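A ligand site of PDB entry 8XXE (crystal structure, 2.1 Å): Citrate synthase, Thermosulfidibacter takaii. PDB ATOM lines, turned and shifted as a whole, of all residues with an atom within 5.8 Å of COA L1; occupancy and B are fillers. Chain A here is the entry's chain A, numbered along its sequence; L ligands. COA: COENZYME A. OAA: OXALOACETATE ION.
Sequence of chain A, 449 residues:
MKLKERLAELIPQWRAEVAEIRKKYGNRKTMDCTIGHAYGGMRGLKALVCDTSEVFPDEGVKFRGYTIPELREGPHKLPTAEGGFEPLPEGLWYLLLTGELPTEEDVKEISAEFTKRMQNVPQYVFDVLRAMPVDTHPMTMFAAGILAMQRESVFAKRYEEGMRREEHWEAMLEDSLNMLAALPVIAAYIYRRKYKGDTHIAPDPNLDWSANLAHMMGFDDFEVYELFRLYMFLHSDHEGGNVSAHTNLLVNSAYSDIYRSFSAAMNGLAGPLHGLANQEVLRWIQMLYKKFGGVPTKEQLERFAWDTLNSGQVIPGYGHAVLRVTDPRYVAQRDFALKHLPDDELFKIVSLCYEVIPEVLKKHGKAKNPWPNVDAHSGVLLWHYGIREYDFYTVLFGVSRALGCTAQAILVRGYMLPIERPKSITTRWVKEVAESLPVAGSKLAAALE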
ATOM      1  N   ARG A  43       6.060  17.619 -38.715  1.00  0.00           N
ATOM      2  CA  ARG A  43       7.391  17.650 -38.116  1.00  0.00           C
ATOM      3  C   ARG A  43       8.340  18.480 -38.977  1.00  0.00           C
ATOM      4  O   ARG A  43       8.491  18.172 -40.151  1.00  0.00           O
ATOM      5  CB  ARG A  43       7.980  16.251 -37.980  1.00  0.00           C
ATOM      6  CG  ARG A  43       9.019  16.126 -36.874  1.00  0.00           C
ATOM      7  CD  ARG A  43       8.414  16.369 -35.489  1.00  0.00           C
ATOM      8  NE  ARG A  43       6.989  16.030 -35.472  1.00  0.00           N
ATOM      9  CZ  ARG A  43       6.460  14.948 -34.900  1.00  0.00           C
ATOM     10  NH1 ARG A  43       7.072  14.391 -33.875  1.00  0.00           N
ATOM     11  NH2 ARG A  43       5.291  14.471 -35.327  1.00  0.00           N
ATOM     12  N   ALA A 277       5.174  12.248 -19.305  1.00  0.00           N
ATOM     13  CA  ALA A 277       6.555  11.745 -19.311  1.00  0.00           C
ATOM     14  C   ALA A 277       7.215  11.783 -17.924  1.00  0.00           C
ATOM     15  O   ALA A 277       7.935  10.866 -17.574  1.00  0.00           O
ATOM     16  CB  ALA A 277       7.356  12.538 -20.305  1.00  0.00           C
ATOM     17  N   GLU A 280       6.071   8.808 -15.882  1.00  0.00           N
ATOM     18  CA  GLU A 280       6.595   7.567 -16.429  1.00  0.00           C
ATOM     19  C   GLU A 280       8.035   7.404 -15.953  1.00  0.00           C
ATOM     20  O   GLU A 280       8.396   6.319 -15.512  1.00  0.00           O
ATOM     21  CB  GLU A 280       6.541   7.513 -17.969  1.00  0.00           C
ATOM     22  CG  GLU A 280       5.219   6.958 -18.490  1.00  0.00           C
ATOM     23  CD  GLU A 280       4.752   7.392 -19.883  1.00  0.00           C
ATOM     24  OE1 GLU A 280       3.649   6.935 -20.268  1.00  0.00           O
ATOM     25  OE2 GLU A 280       5.462   8.182 -20.573  1.00  0.00           O
ATOM     26  N   VAL A 281       8.804   8.488 -16.013  1.00  0.00           N
ATOM     27  CA  VAL A 281      10.201   8.448 -15.607  1.00  0.00           C
ATOM     28  C   VAL A 281      10.265   8.065 -14.137  1.00  0.00           C
ATOM     29  O   VAL A 281      10.954   7.118 -13.794  1.00  0.00           O
ATOM     30  CB  VAL A 281      10.944   9.761 -15.906  1.00  0.00           C
ATOM     31  CG1 VAL A 281      12.258   9.884 -15.129  1.00  0.00           C
ATOM     32  CG2 VAL A 281      11.228   9.929 -17.381  1.00  0.00           C
ATOM     33  N   LEU A 309      16.081  -1.930 -24.416  1.00  0.00           N
ATOM     34  CA  LEU A 309      16.035  -1.549 -25.828  1.00  0.00           C
ATOM     35  C   LEU A 309      15.865  -2.774 -26.734  1.00  0.00           C
ATOM     36  O   LEU A 309      15.010  -2.786 -27.619  1.00  0.00           O
ATOM     37  CB  LEU A 309      17.341  -0.798 -26.145  1.00  0.00           C
ATOM     38  CG  LEU A 309      17.544   0.492 -25.362  1.00  0.00           C
ATOM     39  CD1 LEU A 309      18.938   1.059 -25.577  1.00  0.00           C
ATOM     40  CD2 LEU A 309      16.473   1.506 -25.761  1.00  0.00           C
ATOM     41  N   GLN A 313      11.661  -1.802 -25.894  1.00  0.00           N
ATOM     42  CA  GLN A 313      11.125  -0.775 -25.011  1.00  0.00           C
ATOM     43  C   GLN A 313      11.883   0.534 -25.201  1.00  0.00           C
ATOM     44  O   GLN A 313      13.003   0.560 -25.725  1.00  0.00           O
ATOM     45  CB  GLN A 313      11.148  -1.218 -23.548  1.00  0.00           C
ATOM     46  CG  GLN A 313      10.452  -2.550 -23.277  1.00  0.00           C
ATOM     47  CD  GLN A 313       8.947  -2.522 -23.436  1.00  0.00           C
ATOM     48  OE1 GLN A 313       8.201  -2.723 -22.485  1.00  0.00           O
ATOM     49  NE2 GLN A 313       8.495  -2.305 -24.668  1.00  0.00           N
ATOM     50  N   VAL A 314      11.216   1.618 -24.763  1.00  0.00           N
ATOM     51  CA  VAL A 314      11.803   2.954 -24.716  1.00  0.00           C
ATOM     52  C   VAL A 314      12.321   3.240 -23.300  1.00  0.00           C
ATOM     53  O   VAL A 314      11.671   2.890 -22.328  1.00  0.00           O
ATOM     54  CB  VAL A 314      10.792   4.023 -25.182  1.00  0.00           C
ATOM     55  CG1 VAL A 314      10.378   3.820 -26.639  1.00  0.00           C
ATOM     56  CG2 VAL A 314       9.562   4.108 -24.265  1.00  0.00           C
ATOM     57  N   ILE A 315      13.492   3.892 -23.209  1.00  0.00           N
ATOM     58  CA  ILE A 315      14.021   4.456 -21.974  1.00  0.00           C
ATOM     59  C   ILE A 315      13.408   5.837 -21.693  1.00  0.00           C
ATOM     60  O   ILE A 315      13.770   6.840 -22.317  1.00  0.00           O
ATOM     61  CB  ILE A 315      15.551   4.539 -22.067  1.00  0.00           C
ATOM     62  CG1 ILE A 315      16.159   3.140 -22.166  1.00  0.00           C
ATOM     63  CG2 ILE A 315      16.127   5.327 -20.900  1.00  0.00           C
ATOM     64  CD1 ILE A 315      17.666   3.137 -22.138  1.00  0.00           C
ATOM     65  N   PRO A 316      12.512   5.992 -20.677  1.00  0.00           N
ATOM     66  CA  PRO A 316      11.837   7.287 -20.492  1.00  0.00           C
ATOM     67  C   PRO A 316      12.798   8.390 -20.020  1.00  0.00           C
ATOM     68  O   PRO A 316      13.740   8.140 -19.279  1.00  0.00           O
ATOM     69  CB  PRO A 316      10.704   6.940 -19.505  1.00  0.00           C
ATOM     70  CG  PRO A 316      11.246   5.762 -18.718  1.00  0.00           C
ATOM     71  CD  PRO A 316      12.119   4.984 -19.686  1.00  0.00           C
ATOM     72  N   GLY A 317      12.557   9.600 -20.524  1.00  0.00           N
ATOM     73  CA  GLY A 317      13.259  10.802 -20.094  1.00  0.00           C
ATOM     74  C   GLY A 317      14.455  11.116 -20.990  1.00  0.00           C
ATOM     75  O   GLY A 317      15.191  12.054 -20.717  1.00  0.00           O
ATOM     76  N   TYR A 318      14.656  10.261 -22.012  1.00  0.00           N
ATOM     77  CA  TYR A 318      15.700  10.457 -23.003  1.00  0.00           C
ATOM     78  C   TYR A 318      15.047  10.608 -24.383  1.00  0.00           C
ATOM     79  O   TYR A 318      13.983  10.046 -24.647  1.00  0.00           O
ATOM     80  CB  TYR A 318      16.740   9.342 -22.847  1.00  0.00           C
ATOM     81  CG  TYR A 318      17.555   9.458 -21.578  1.00  0.00           C
ATOM     82  CD1 TYR A 318      17.001   9.167 -20.334  1.00  0.00           C
ATOM     83  CD2 TYR A 318      18.853   9.946 -21.612  1.00  0.00           C
ATOM     84  CE1 TYR A 318      17.750   9.317 -19.167  1.00  0.00           C
ATOM     85  CE2 TYR A 318      19.600  10.106 -20.465  1.00  0.00           C
ATOM     86  CZ  TYR A 318      19.045   9.796 -19.231  1.00  0.00           C
ATOM     87  OH  TYR A 318      19.808   9.997 -18.104  1.00  0.00           O
ATOM     88  N   GLY A 319      15.656  11.453 -25.219  1.00  0.00           N
ATOM     89  CA  GLY A 319      15.119  11.764 -26.547  1.00  0.00           C
ATOM     90  C   GLY A 319      14.171  12.962 -26.531  1.00  0.00           C
ATOM     91  O   GLY A 319      13.564  13.301 -25.516  1.00  0.00           O
ATOM     92  N   HIS A 320      14.041  13.582 -27.710  1.00  0.00           N
ATOM     93  CA  HIS A 320      13.077  14.649 -27.909  1.00  0.00           C
ATOM     94  C   HIS A 320      12.704  14.739 -29.390  1.00  0.00           C
ATOM     95  O   HIS A 320      13.503  14.395 -30.249  1.00  0.00           O
ATOM     96  CB  HIS A 320      13.649  15.998 -27.446  1.00  0.00           C
ATOM     97  CG  HIS A 320      12.626  16.999 -27.034  1.00  0.00           C
ATOM     98  ND1 HIS A 320      12.205  18.040 -27.853  1.00  0.00           N
ATOM     99  CD2 HIS A 320      11.921  17.120 -25.883  1.00  0.00           C
ATOM    100  CE1 HIS A 320      11.280  18.751 -27.203  1.00  0.00           C
ATOM    101  NE2 HIS A 320      11.108  18.226 -26.000  1.00  0.00           N
ATOM    102  N   ALA A 321      11.501  15.275 -29.639  1.00  0.00           N
ATOM    103  CA  ALA A 321      10.983  15.546 -30.972  1.00  0.00           C
ATOM    104  C   ALA A 321      11.754  16.648 -31.697  1.00  0.00           C
ATOM    105  O   ALA A 321      11.481  16.855 -32.874  1.00  0.00           O
ATOM    106  CB  ALA A 321       9.516  15.904 -30.880  1.00  0.00           C
ATOM    107  N   VAL A 322      12.663  17.360 -30.993  1.00  0.00           N
ATOM    108  CA  VAL A 322      13.417  18.487 -31.614  1.00  0.00           C
ATOM    109  C   VAL A 322      14.803  18.627 -30.967  1.00  0.00           C
ATOM    110  O   VAL A 322      15.789  18.742 -31.722  1.00  0.00           O
ATOM    111  CB  VAL A 322      12.626  19.805 -31.533  1.00  0.00           C
ATOM    112  CG1 VAL A 322      11.550  19.805 -30.458  1.00  0.00           C
ATOM    113  CG2 VAL A 322      13.517  21.033 -31.421  1.00  0.00           C
ATOM    114  N   ARG A 324      18.419  18.066 -29.439  1.00  0.00           N
ATOM    115  CA  ARG A 324      19.484  17.211 -29.971  1.00  0.00           C
ATOM    116  C   ARG A 324      20.680  17.136 -29.035  1.00  0.00           C
ATOM    117  O   ARG A 324      21.606  16.379 -29.313  1.00  0.00           O
ATOM    118  CB  ARG A 324      19.937  17.736 -31.334  1.00  0.00           C
ATOM    119  CG  ARG A 324      20.313  16.674 -32.358  1.00  0.00           C
ATOM    120  CD  ARG A 324      19.211  15.685 -32.735  1.00  0.00           C
ATOM    121  NE  ARG A 324      17.856  16.061 -32.324  1.00  0.00           N
ATOM    122  CZ  ARG A 324      16.734  15.589 -32.858  1.00  0.00           C
ATOM    123  NH1 ARG A 324      15.647  15.453 -32.101  1.00  0.00           N
ATOM    124  NH2 ARG A 324      16.737  15.142 -34.099  1.00  0.00           N
ATOM    125  N   ARG A 329      16.982  22.441 -19.186  1.00  0.00           N
ATOM    126  CA  ARG A 329      16.008  22.362 -18.109  1.00  0.00           C
ATOM    127  C   ARG A 329      16.343  21.176 -17.203  1.00  0.00           C
ATOM    128  O   ARG A 329      16.112  21.231 -15.988  1.00  0.00           O
ATOM    129  CB  ARG A 329      14.589  22.289 -18.688  1.00  0.00           C
ATOM    130  CG  ARG A 329      14.198  23.493 -19.554  1.00  0.00           C
ATOM    131  CD  ARG A 329      12.864  23.327 -20.270  1.00  0.00           C
ATOM    132  NE  ARG A 329      12.844  22.131 -21.104  1.00  0.00           N
ATOM    133  CZ  ARG A 329      11.811  21.668 -21.802  1.00  0.00           C
ATOM    134  NH1 ARG A 329      10.623  22.272 -21.768  1.00  0.00           N
ATOM    135  NH2 ARG A 329      11.964  20.580 -22.534  1.00  0.00           N
ATOM    136  N   LEU A 361      22.251   4.631 -25.736  1.00  0.00           N
ATOM    137  CA  LEU A 361      21.300   5.053 -26.751  1.00  0.00           C
ATOM    138  C   LEU A 361      22.016   5.449 -28.053  1.00  0.00           C
ATOM    139  O   LEU A 361      21.409   5.357 -29.126  1.00  0.00           O
ATOM    140  CB  LEU A 361      20.474   6.231 -26.207  1.00  0.00           C
ATOM    141  CG  LEU A 361      19.374   5.863 -25.205  1.00  0.00           C
ATOM    142  CD1 LEU A 361      18.800   7.120 -24.570  1.00  0.00           C
ATOM    143  CD2 LEU A 361      18.257   5.078 -25.884  1.00  0.00           C
ATOM    144  N   HIS A 364      23.024   1.957 -29.667  1.00  0.00           N
ATOM    145  CA  HIS A 364      21.777   1.382 -30.159  1.00  0.00           C
ATOM    146  C   HIS A 364      21.328   2.073 -31.453  1.00  0.00           C
ATOM    147  O   HIS A 364      20.720   1.432 -32.316  1.00  0.00           O
ATOM    148  CB  HIS A 364      20.716   1.401 -29.045  1.00  0.00           C
ATOM    149  CG  HIS A 364      19.348   0.951 -29.444  1.00  0.00           C
ATOM    150  ND1 HIS A 364      18.259   1.789 -29.475  1.00  0.00           N
ATOM    151  CD2 HIS A 364      18.888  -0.261 -29.806  1.00  0.00           C
ATOM    152  CE1 HIS A 364      17.176   1.110 -29.821  1.00  0.00           C
ATOM    153  NE2 HIS A 364      17.533  -0.148 -30.032  1.00  0.00           N
ATOM    154  N   LYS A 366      19.092   4.241 -32.707  1.00  0.00           N
ATOM    155  CA  LYS A 366      17.750   4.545 -33.190  1.00  0.00           C
ATOM    156  C   LYS A 366      17.278   5.942 -32.755  1.00  0.00           C
ATOM    157  O   LYS A 366      16.627   6.628 -33.528  1.00  0.00           O
ATOM    158  CB  LYS A 366      16.675   3.559 -32.682  1.00  0.00           C
ATOM    159  CG  LYS A 366      17.003   2.076 -32.777  1.00  0.00           C
ATOM    160  CD  LYS A 366      16.453   1.319 -33.966  1.00  0.00           C
ATOM    161  CE  LYS A 366      16.503  -0.182 -33.722  1.00  0.00           C
ATOM    162  NZ  LYS A 366      16.049  -0.979 -34.885  1.00  0.00           N
ATOM    163  N   ALA A 367      17.551   6.322 -31.494  1.00  0.00           N
ATOM    164  CA  ALA A 367      17.182   7.636 -30.986  1.00  0.00           C
ATOM    165  C   ALA A 367      17.980   8.710 -31.736  1.00  0.00           C
ATOM    166  O   ALA A 367      19.199   8.619 -31.834  1.00  0.00           O
ATOM    167  CB  ALA A 367      17.412   7.725 -29.488  1.00  0.00           C
ATOM    168  N   LYS A 368      17.273   9.725 -32.275  1.00  0.00           N
ATOM    169  CA  LYS A 368      17.957  10.861 -32.886  1.00  0.00           C
ATOM    170  C   LYS A 368      18.695  11.644 -31.792  1.00  0.00           C
ATOM    171  O   LYS A 368      19.748  12.220 -32.062  1.00  0.00           O
ATOM    172  CB  LYS A 368      16.965  11.704 -33.697  1.00  0.00           C
ATOM    173  N   ASN A 369      18.166  11.624 -30.550  1.00  0.00           N
ATOM    174  CA  ASN A 369      18.688  12.383 -29.417  1.00  0.00           C
ATOM    175  C   ASN A 369      18.937  11.463 -28.217  1.00  0.00           C
ATOM    176  O   ASN A 369      17.974  11.012 -27.560  1.00  0.00           O
ATOM    177  CB  ASN A 369      17.732  13.525 -29.019  1.00  0.00           C
ATOM    178  CG  ASN A 369      18.106  14.204 -27.718  1.00  0.00           C
ATOM    179  OD1 ASN A 369      19.282  14.313 -27.358  1.00  0.00           O
ATOM    180  ND2 ASN A 369      17.102  14.711 -27.006  1.00  0.00           N
ATOM    181  N   ASN A 373      15.844  14.792 -21.339  1.00  0.00           N
ATOM    182  CA  ASN A 373      15.006  15.975 -21.409  1.00  0.00           C
ATOM    183  C   ASN A 373      14.562  16.409 -19.998  1.00  0.00           C
ATOM    184  O   ASN A 373      14.872  15.779 -18.975  1.00  0.00           O
ATOM    185  CB  ASN A 373      13.831  15.712 -22.372  1.00  0.00           C
ATOM    186  CG  ASN A 373      13.004  14.504 -22.007  1.00  0.00           C
ATOM    187  OD1 ASN A 373      12.500  14.410 -20.892  1.00  0.00           O
ATOM    188  ND2 ASN A 373      12.889  13.551 -22.920  1.00  0.00           N
ATOM    189  N   VAL A 374      13.764  17.487 -19.926  1.00  0.00           N
ATOM    190  CA  VAL A 374      13.331  18.037 -18.643  1.00  0.00           C
ATOM    191  C   VAL A 374      12.660  16.971 -17.778  1.00  0.00           C
ATOM    192  O   VAL A 374      12.894  16.961 -16.558  1.00  0.00           O
ATOM    193  CB  VAL A 374      12.417  19.258 -18.893  1.00  0.00           C
ATOM    194  CG1 VAL A 374      11.151  18.894 -19.656  1.00  0.00           C
ATOM    195  CG2 VAL A 374      12.075  19.978 -17.585  1.00  0.00           C
ATOM    196  N   ASP A 375      11.937  16.018 -18.407  1.00  0.00           N
ATOM    197  CA  ASP A 375      11.104  15.065 -17.677  1.00  0.00           C
ATOM    198  C   ASP A 375      11.902  13.964 -16.992  1.00  0.00           C
ATOM    199  O   ASP A 375      11.372  13.221 -16.154  1.00  0.00           O
ATOM    200  CB  ASP A 375      10.032  14.500 -18.596  1.00  0.00           C
ATOM    201  CG  ASP A 375       9.200  15.608 -19.225  1.00  0.00           C
ATOM    202  OD1 ASP A 375       8.643  16.459 -18.448  1.00  0.00           O
ATOM    203  OD2 ASP A 375       9.120  15.652 -20.495  1.00  0.00           O
HETATM  204  N1A COA L   1      14.382   4.947 -25.831  1.00  0.00           N
HETATM  205  C2A COA L   1      14.272   4.068 -26.842  1.00  0.00           C
HETATM  206  N3A COA L   1      14.044   4.291 -28.135  1.00  0.00           N
HETATM  207  C4A COA L   1      13.935   5.612 -28.389  1.00  0.00           C
HETATM  208  C5A COA L   1      14.020   6.634 -27.469  1.00  0.00           C
HETATM  209  C6A COA L   1      14.248   6.269 -26.121  1.00  0.00           C
HETATM  210  N6A COA L   1      14.343   7.159 -25.138  1.00  0.00           N
HETATM  211  N7A COA L   1      13.833   7.870 -28.090  1.00  0.00           N
HETATM  212  C8A COA L   1      13.659   7.582 -29.350  1.00  0.00           C
HETATM  213  N9A COA L   1      13.720   6.212 -29.607  1.00  0.00           N
HETATM  214  C1B COA L   1      13.536   5.545 -30.913  1.00  0.00           C
HETATM  215  C2B COA L   1      12.144   5.743 -31.484  1.00  0.00           C
HETATM  216  O2B COA L   1      11.182   4.913 -30.873  1.00  0.00           O
HETATM  217  C3B COA L   1      12.385   5.439 -32.963  1.00  0.00           C
HETATM  218  O3B COA L   1      12.402   4.040 -33.256  1.00  0.00           O
HETATM  219  P3B COA L   1      11.322   3.564 -34.372  1.00  0.00           P
HETATM  220  O7A COA L   1       9.928   3.946 -33.875  1.00  0.00           O
HETATM  221  O8A COA L   1      11.483   2.061 -34.506  1.00  0.00           O
HETATM  222  O9A COA L   1      11.691   4.305 -35.653  1.00  0.00           O
HETATM  223  C4B COA L   1      13.777   6.047 -33.187  1.00  0.00           C
HETATM  224  O4B COA L   1      14.396   6.118 -31.874  1.00  0.00           O
HETATM  225  C5B COA L   1      13.754   7.396 -33.845  1.00  0.00           C
HETATM  226  O5B COA L   1      12.845   8.285 -33.130  1.00  0.00           O
HETATM  227  P1A COA L   1      13.302   9.809 -32.826  1.00  0.00           P
HETATM  228  O1A COA L   1      13.189  10.612 -34.080  1.00  0.00           O
HETATM  229  O2A COA L   1      14.642   9.818 -32.168  1.00  0.00           O
HETATM  230  O3A COA L   1      12.133  10.220 -31.782  1.00  0.00           O
HETATM  231  P2A COA L   1      10.628  10.778 -31.939  1.00  0.00           P
HETATM  232  O4A COA L   1      10.720  12.244 -32.255  1.00  0.00           O
HETATM  233  O5A COA L   1       9.789   9.905 -32.822  1.00  0.00           O
HETATM  234  O6A COA L   1      10.086  10.597 -30.440  1.00  0.00           O
HETATM  235  CBP COA L   1      10.014  11.054 -28.058  1.00  0.00           C
HETATM  236  CCP COA L   1      10.385  11.618 -29.428  1.00  0.00           C
HETATM  237  CDP COA L   1      10.278  12.143 -26.998  1.00  0.00           C
HETATM  238  CEP COA L   1       8.517  10.705 -28.062  1.00  0.00           C
HETATM  239  CAP COA L   1      10.853   9.791 -27.769  1.00  0.00           C
HETATM  240  OAP COA L   1      12.250  10.175 -27.689  1.00  0.00           O
HETATM  241  C9P COA L   1      10.410   9.001 -26.520  1.00  0.00           C
HETATM  242  O9P COA L   1       9.542   8.134 -26.640  1.00  0.00           O
HETATM  243  N8P COA L   1      10.987   9.277 -25.344  1.00  0.00           N
HETATM  244  C7P COA L   1      10.632   8.638 -24.090  1.00  0.00           C
HETATM  245  C6P COA L   1       9.485   9.344 -23.371  1.00  0.00           C
HETATM  246  C5P COA L   1       9.823  10.783 -22.983  1.00  0.00           C
HETATM  247  O5P COA L   1      10.786  11.023 -22.245  1.00  0.00           O
HETATM  248  N4P COA L   1       9.049  11.757 -23.505  1.00  0.00           N
HETATM  249  C3P COA L   1       9.145  13.163 -23.127  1.00  0.00           C
HETATM  250  C2P COA L   1       9.392  14.108 -24.313  1.00  0.00           C
HETATM  251  S1P COA L   1       9.617  15.842 -23.827  1.00  0.00           S
HETATM  252  O1  OAA L   2       8.284  20.882 -26.902  1.00  0.00           O
HETATM  253  O2  OAA L   2       7.662  19.124 -28.093  1.00  0.00           O
HETATM  254  O4  OAA L   2       7.851  21.326 -22.927  1.00  0.00           O
HETATM  255  O5  OAA L   2       6.237  21.058 -24.386  1.00  0.00           O
HETATM  256  O3  OAA L   2       9.180  19.425 -24.185  1.00  0.00           O
HETATM  257  C1  OAA L   2       7.828  19.710 -27.000  1.00  0.00           C
HETATM  258  C2  OAA L   2       7.460  18.969 -25.709  1.00  0.00           C
HETATM  259  C3  OAA L   2       8.030  19.716 -24.523  1.00  0.00           C
HETATM  260  C4  OAA L   2       7.356  20.722 -23.915  1.00  0.00           C
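The backbone NH (N) of His 320 sits close to the side-chain amide nitrogen (ND2) of Asn 369, at 3.3 Å.
O of Gly 319 lies within hydrogen-bond range of ND2 of Asn 373.
The backbone NH (N) of Val 322 lies close to a ring nitrogen (ND1) of His 320 (3.2 Å).
The backbone carbonyl oxygen of Asn 369 lies close to the backbone NH of Gly 319, 3.3 Å away.
OD1 of Asn 373 is in hydrogen-bond range of N of Asp 375 (3.0 Å).
The backbone carbonyl oxygen of Gly 317 sits at hydrogen-bond distance from the backbone NH of Asn 373, at 2.9 Å.
O of His 320 lies within hydrogen-bond range of NH1 of Arg 324 (3.0 Å).
A ring nitrogen (NE2) of His 320 sits close to a sulfur (S1P) of COA L1 (3.6 Å).
The backbone NH (N) of Ala 367 lies within hydrogen-bond range of an oxygen (O4B) of COA L1, 3.2 Å away.
The backbone carbonyl oxygen (O) of Tyr 318 lies within hydrogen-bond range of a nitrogen (N6A) of COA L1 (3.0 Å).
O of Ile 315 is in hydrogen-bond range of N6A of COA L1, 2.9 Å away.
The backbone NH (N) of Gly 317 sits at hydrogen-bond distance from an oxygen (O5P) of COA L1 (2.9 Å).
The backbone NH (N) of Ile 315 lies within hydrogen-bond range of a nitrogen (N1A) of COA L1 (3.0 Å).
O3 of OAA L2 sits at hydrogen-bond distance from NE2 of His 320, 2.9 Å away.
The guanidinium group (NH1) of Arg 329 lies within salt-bridge range of an oxygen (O4) of OAA L2 (3.1 Å).
S1P of COA L1 sits close to OD2 of Asp 375, 3.4 Å away.
The side-chain amide nitrogen of Asn 373 sits at hydrogen-bond distance from an oxygen (O5P) of COA L1 (3.4 Å).
N of Lys 368 lies within hydrogen-bond range of O2A of COA L1, 2.6 Å away.
An oxygen (O3) of OAA L2 sits close to a sulfur (S1P) of COA L1, 3.6 Å away.
The backbone carbonyl oxygen of Lys 366 lies close to an oxygen (O4B) of COA L1 (2.8 Å).
Merely in contact with COA L1: Ala 277 (3.4 Å), Leu 309 (3.5 Å), Gln 313 (3.9 Å), Val 314 (3.4 Å), Pro 316 (3.99 Å), Gly 319 (3.5 Å), Ala 321 (3.6 Å) and Leu 361 (3.9 Å).
Hydrophobic or aromatic side chains within 4 Å of COA L1: Ala 277, Leu 309, Val 314, Ile 315, Tyr 318, His 320, Leu 361 and Ala 367.
Of the 26 residues printed, 17 come within 4 Å of COA L1.
The nearest printed residue that does not touch COA L1 is Asn 369 (4.3 Å).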
